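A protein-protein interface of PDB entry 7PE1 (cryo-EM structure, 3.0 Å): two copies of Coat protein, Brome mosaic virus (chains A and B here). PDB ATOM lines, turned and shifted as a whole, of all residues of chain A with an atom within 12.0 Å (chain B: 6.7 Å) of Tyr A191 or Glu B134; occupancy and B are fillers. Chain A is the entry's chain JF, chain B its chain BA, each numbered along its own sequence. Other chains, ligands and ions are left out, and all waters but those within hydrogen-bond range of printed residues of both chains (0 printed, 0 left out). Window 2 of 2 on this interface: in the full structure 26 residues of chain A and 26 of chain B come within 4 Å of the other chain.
O of Val A190 touches CG1 of Val B135, 3.7 Å away. Tyr A191 touches Ala B39 (CE2 to O, 3.8 Å). CE2 of Tyr A191 touches CA of Ala B40 (3.97 Å). CE1 of Tyr A191 touches CG of Glu B134, at 3.5 Å. Tyr A191 touches Val B135. Lys A192 touches Ala B40 (O to CB, 3.2 Å).
O of Pro A189 sits at hydrogen-bond distance from NZ of Lys A192 (3.0 Å). The side-chain amide oxygen (OE1) of Gln B42 lies within hydrogen-bond range of the backbone NH (N) of Ala B39 (2.8 Å).
No position is printed for both chains. Of the 8 pairs that touch across the chains among the printed residues, none has its exchanged pair printed and touching as well.
Of the printed residues of chain B, Val A190 touches Val B135. Of chain B, only Ala B39, Ala B40, Gly B41, Glu B134 and Val B135 come within 4 Å of Tyr A191. Of the printed residues of chain B, Lys A192 touches Ala B40 (3.2 Å) and Gly B41 (3.3 Å). Ile B38 touches none of the printed residues of chain A. Of chain A, only Tyr A191 (3.8 Å) comes within 4 Å of Ala B39. Ala B40 touches two residues of chain A. Ser B132 touches none of the printed residues of chain A. No residue of chain A comes within 4 Å of Lys B133. Of the printed residues of chain A, Glu B134 touches Tyr A191. Of chain A, only Val A190 and Tyr A191 come within 4 Å of Val B135. The nearest residue of chain B that does not touch Tyr A191 is Ile B38 (4.1 Å).
Hydrophobic or aromatic side chains of chain A that line the printed part of chain B: Val A190 and Tyr A191.
N of Gly B41 sits at hydrogen-bond distance from O of Tyr A191 (2.8 Å). N of Gly B41 lies within hydrogen-bond range of O of Lys A192 (3.3 Å).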
ATOM      1  N   PHE A 187       1.961 -24.208  -0.763  1.00  0.00           N
ATOM      2  CA  PHE A 187       2.554 -23.357   0.253  1.00  0.00           C
ATOM      3  C   PHE A 187       2.644 -21.927  -0.260  1.00  0.00           C
ATOM      4  O   PHE A 187       2.759 -21.685  -1.463  1.00  0.00           O
ATOM      5  CB  PHE A 187       3.951 -23.854   0.634  1.00  0.00           C
ATOM      6  CG  PHE A 187       3.958 -24.947   1.663  1.00  0.00           C
ATOM      7  CD1 PHE A 187       3.612 -24.683   2.974  1.00  0.00           C
ATOM      8  CD2 PHE A 187       4.347 -26.231   1.326  1.00  0.00           C
ATOM      9  CE1 PHE A 187       3.630 -25.687   3.926  1.00  0.00           C
ATOM     10  CE2 PHE A 187       4.367 -27.234   2.273  1.00  0.00           C
ATOM     11  CZ  PHE A 187       4.010 -26.962   3.573  1.00  0.00           C
ATOM     12  N   THR A 188       2.584 -20.978   0.664  1.00  0.00           N
ATOM     13  CA  THR A 188       2.761 -19.580   0.305  1.00  0.00           C
ATOM     14  C   THR A 188       4.210 -19.327  -0.110  1.00  0.00           C
ATOM     15  O   THR A 188       5.135 -19.831   0.536  1.00  0.00           O
ATOM     16  CB  THR A 188       2.378 -18.684   1.484  1.00  0.00           C
ATOM     17  OG1 THR A 188       0.997 -18.883   1.809  1.00  0.00           O
ATOM     18  CG2 THR A 188       2.593 -17.230   1.156  1.00  0.00           C
ATOM     19  N   PRO A 189       4.442 -18.582  -1.193  1.00  0.00           N
ATOM     20  CA  PRO A 189       5.822 -18.262  -1.587  1.00  0.00           C
ATOM     21  C   PRO A 189       6.546 -17.487  -0.495  1.00  0.00           C
ATOM     22  O   PRO A 189       5.981 -16.593   0.136  1.00  0.00           O
ATOM     23  CB  PRO A 189       5.646 -17.425  -2.858  1.00  0.00           C
ATOM     24  CG  PRO A 189       4.231 -16.946  -2.812  1.00  0.00           C
ATOM     25  CD  PRO A 189       3.461 -18.032  -2.141  1.00  0.00           C
ATOM     26  N   VAL A 190       7.820 -17.833  -0.288  1.00  0.00           N
ATOM     27  CA  VAL A 190       8.529 -17.381   0.906  1.00  0.00           C
ATOM     28  C   VAL A 190       8.997 -15.940   0.758  1.00  0.00           C
ATOM     29  O   VAL A 190       9.213 -15.241   1.753  1.00  0.00           O
ATOM     30  CB  VAL A 190       9.704 -18.328   1.221  1.00  0.00           C
ATOM     31  CG1 VAL A 190       9.196 -19.734   1.480  1.00  0.00           C
ATOM     32  CG2 VAL A 190      10.709 -18.324   0.089  1.00  0.00           C
ATOM     33  N   TYR A 191       9.178 -15.475  -0.472  1.00  0.00           N
ATOM     34  CA  TYR A 191       9.696 -14.129  -0.706  1.00  0.00           C
ATOM     35  C   TYR A 191       8.531 -13.142  -0.675  1.00  0.00           C
ATOM     36  O   TYR A 191       7.980 -12.762  -1.707  1.00  0.00           O
ATOM     37  CB  TYR A 191      10.459 -14.079  -2.022  1.00  0.00           C
ATOM     38  CG  TYR A 191      11.311 -12.848  -2.196  1.00  0.00           C
ATOM     39  CD1 TYR A 191      12.139 -12.404  -1.176  1.00  0.00           C
ATOM     40  CD2 TYR A 191      11.302 -12.138  -3.387  1.00  0.00           C
ATOM     41  CE1 TYR A 191      12.922 -11.280  -1.334  1.00  0.00           C
ATOM     42  CE2 TYR A 191      12.078 -11.016  -3.553  1.00  0.00           C
ATOM     43  CZ  TYR A 191      12.887 -10.590  -2.524  1.00  0.00           C
ATOM     44  OH  TYR A 191      13.664  -9.468  -2.694  1.00  0.00           O
ATOM     45  N   LYS A 192       8.158 -12.719   0.529  1.00  0.00           N
ATOM     46  CA  LYS A 192       7.032 -11.806   0.724  1.00  0.00           C
ATOM     47  C   LYS A 192       7.306 -10.414   0.178  1.00  0.00           C
ATOM     48  O   LYS A 192       7.083 -10.145  -0.998  1.00  0.00           O
ATOM     49  CB  LYS A 192       6.676 -11.699   2.207  1.00  0.00           C
ATOM     50  CG  LYS A 192       6.019 -12.928   2.776  1.00  0.00           C
ATOM     51  CD  LYS A 192       4.736 -13.243   2.039  1.00  0.00           C
ATOM     52  CE  LYS A 192       4.052 -14.435   2.657  1.00  0.00           C
ATOM     53  NZ  LYS A 192       4.979 -15.592   2.753  1.00  0.00           N
ATOM     54  OXT LYS A 192       7.748  -9.524   0.903  1.00  0.00           O
ATOM     55  N   ILE B  38      14.296 -10.027  -9.563  1.00  0.00           N
ATOM     56  CA  ILE B  38      13.028 -10.614  -9.150  1.00  0.00           C
ATOM     57  C   ILE B  38      12.313  -9.629  -8.237  1.00  0.00           C
ATOM     58  O   ILE B  38      12.918  -9.094  -7.302  1.00  0.00           O
ATOM     59  CB  ILE B  38      13.234 -11.968  -8.441  1.00  0.00           C
ATOM     60  CG1 ILE B  38      13.376 -13.095  -9.460  1.00  0.00           C
ATOM     61  CG2 ILE B  38      12.098 -12.277  -7.489  1.00  0.00           C
ATOM     62  CD1 ILE B  38      13.397 -14.464  -8.835  1.00  0.00           C
ATOM     63  N   ALA B  39      11.035  -9.383  -8.513  1.00  0.00           N
ATOM     64  CA  ALA B  39      10.199  -8.552  -7.664  1.00  0.00           C
ATOM     65  C   ALA B  39       9.646  -9.362  -6.496  1.00  0.00           C
ATOM     66  O   ALA B  39       9.680 -10.592  -6.484  1.00  0.00           O
ATOM     67  CB  ALA B  39       9.056  -7.939  -8.470  1.00  0.00           C
ATOM     68  N   ALA B  40       9.121  -8.650  -5.504  1.00  0.00           N
ATOM     69  CA  ALA B  40       8.576  -9.307  -4.326  1.00  0.00           C
ATOM     70  C   ALA B  40       7.390 -10.187  -4.698  1.00  0.00           C
ATOM     71  O   ALA B  40       6.554  -9.819  -5.525  1.00  0.00           O
ATOM     72  CB  ALA B  40       8.160  -8.267  -3.292  1.00  0.00           C
ATOM     73  N   GLY B  41       7.330 -11.367  -4.089  1.00  0.00           N
ATOM     74  CA  GLY B  41       6.249 -12.298  -4.344  1.00  0.00           C
ATOM     75  C   GLY B  41       6.212 -12.868  -5.740  1.00  0.00           C
ATOM     76  O   GLY B  41       5.128 -13.140  -6.259  1.00  0.00           O
ATOM     77  N   GLN B  42       7.368 -13.085  -6.358  1.00  0.00           N
ATOM     78  CA  GLN B  42       7.422 -13.529  -7.742  1.00  0.00           C
ATOM     79  C   GLN B  42       8.025 -14.915  -7.918  1.00  0.00           C
ATOM     80  O   GLN B  42       8.038 -15.425  -9.044  1.00  0.00           O
ATOM     81  CB  GLN B  42       8.205 -12.515  -8.587  1.00  0.00           C
ATOM     82  CG  GLN B  42       7.751 -12.430 -10.028  1.00  0.00           C
ATOM     83  CD  GLN B  42       8.391 -11.278 -10.771  1.00  0.00           C
ATOM     84  OE1 GLN B  42       9.266 -10.595 -10.244  1.00  0.00           O
ATOM     85  NE2 GLN B  42       7.954 -11.054 -12.003  1.00  0.00           N
ATOM     86  N   GLY B  43       8.511 -15.545  -6.850  1.00  0.00           N
ATOM     87  CA  GLY B  43       9.097 -16.864  -6.950  1.00  0.00           C
ATOM     88  C   GLY B  43       8.056 -17.968  -7.020  1.00  0.00           C
ATOM     89  O   GLY B  43       6.851 -17.746  -6.904  1.00  0.00           O
ATOM     90  N   ASP B 130      14.490 -14.713  11.175  1.00  0.00           N
ATOM     91  CA  ASP B 130      15.038 -13.443  11.630  1.00  0.00           C
ATOM     92  C   ASP B 130      14.564 -12.334  10.703  1.00  0.00           C
ATOM     93  O   ASP B 130      14.673 -12.455   9.480  1.00  0.00           O
ATOM     94  CB  ASP B 130      16.565 -13.499  11.669  1.00  0.00           C
ATOM     95  CG  ASP B 130      17.175 -12.297  12.350  1.00  0.00           C
ATOM     96  OD1 ASP B 130      16.418 -11.456  12.871  1.00  0.00           O
ATOM     97  OD2 ASP B 130      18.416 -12.190  12.366  1.00  0.00           O
ATOM     98  N   SER B 131      14.041 -11.256  11.289  1.00  0.00           N
ATOM     99  CA  SER B 131      13.458 -10.171  10.507  1.00  0.00           C
ATOM    100  C   SER B 131      14.496  -9.350   9.756  1.00  0.00           C
ATOM    101  O   SER B 131      14.120  -8.571   8.875  1.00  0.00           O
ATOM    102  CB  SER B 131      12.645  -9.246  11.412  1.00  0.00           C
ATOM    103  OG  SER B 131      13.498  -8.438  12.202  1.00  0.00           O
ATOM    104  N   SER B 132      15.781  -9.503  10.070  1.00  0.00           N
ATOM    105  CA  SER B 132      16.843  -8.750   9.415  1.00  0.00           C
ATOM    106  C   SER B 132      17.489  -9.530   8.275  1.00  0.00           C
ATOM    107  O   SER B 132      18.692  -9.397   8.038  1.00  0.00           O
ATOM    108  CB  SER B 132      17.896  -8.323  10.435  1.00  0.00           C
ATOM    109  OG  SER B 132      18.267  -9.405  11.270  1.00  0.00           O
ATOM    110  N   LYS B 133      16.715 -10.346   7.571  1.00  0.00           N
ATOM    111  CA  LYS B 133      17.175 -11.081   6.401  1.00  0.00           C
ATOM    112  C   LYS B 133      16.311 -10.730   5.194  1.00  0.00           C
ATOM    113  O   LYS B 133      15.332  -9.988   5.291  1.00  0.00           O
ATOM    114  CB  LYS B 133      17.162 -12.591   6.656  1.00  0.00           C
ATOM    115  CG  LYS B 133      18.274 -13.077   7.562  1.00  0.00           C
ATOM    116  CD  LYS B 133      18.420 -14.584   7.492  1.00  0.00           C
ATOM    117  CE  LYS B 133      19.429 -15.087   8.510  1.00  0.00           C
ATOM    118  NZ  LYS B 133      20.748 -14.423   8.354  1.00  0.00           N
ATOM    119  N   GLU B 134      16.697 -11.268   4.040  1.00  0.00           N
ATOM    120  CA  GLU B 134      15.921 -11.051   2.824  1.00  0.00           C
ATOM    121  C   GLU B 134      14.613 -11.832   2.858  1.00  0.00           C
ATOM    122  O   GLU B 134      13.553 -11.294   2.523  1.00  0.00           O
ATOM    123  CB  GLU B 134      16.764 -11.435   1.610  1.00  0.00           C
ATOM    124  CG  GLU B 134      16.071 -11.331   0.267  1.00  0.00           C
ATOM    125  CD  GLU B 134      17.011 -11.651  -0.885  1.00  0.00           C
ATOM    126  OE1 GLU B 134      18.204 -11.912  -0.625  1.00  0.00           O
ATOM    127  OE2 GLU B 134      16.560 -11.637  -2.049  1.00  0.00           O
ATOM    128  N   VAL B 135      14.667 -13.097   3.271  1.00  0.00           N
ATOM    129  CA  VAL B 135      13.491 -13.943   3.432  1.00  0.00           C
ATOM    130  C   VAL B 135      13.264 -14.139   4.923  1.00  0.00           C
ATOM    131  O   VAL B 135      14.102 -14.734   5.609  1.00  0.00           O
ATOM    132  CB  VAL B 135      13.661 -15.295   2.725  1.00  0.00           C
ATOM    133  CG1 VAL B 135      12.544 -16.244   3.115  1.00  0.00           C
ATOM    134  CG2 VAL B 135      13.703 -15.114   1.226  1.00  0.00           C
ATOM    135  N   VAL B 136      12.138 -13.636   5.429  1.00  0.00           N
ATOM    136  CA  VAL B 136      11.812 -13.772   6.844  1.00  0.00           C
ATOM    137  C   VAL B 136      10.870 -14.951   7.038  1.00  0.00           C
ATOM    138  O   VAL B 136       9.647 -14.781   7.097  1.00  0.00           O
ATOM    139  CB  VAL B 136      11.202 -12.471   7.391  1.00  0.00           C
ATOM    140  CG1 VAL B 136      11.072 -12.528   8.896  1.00  0.00           C
ATOM    141  CG2 VAL B 136      12.049 -11.285   6.975  1.00  0.00           C
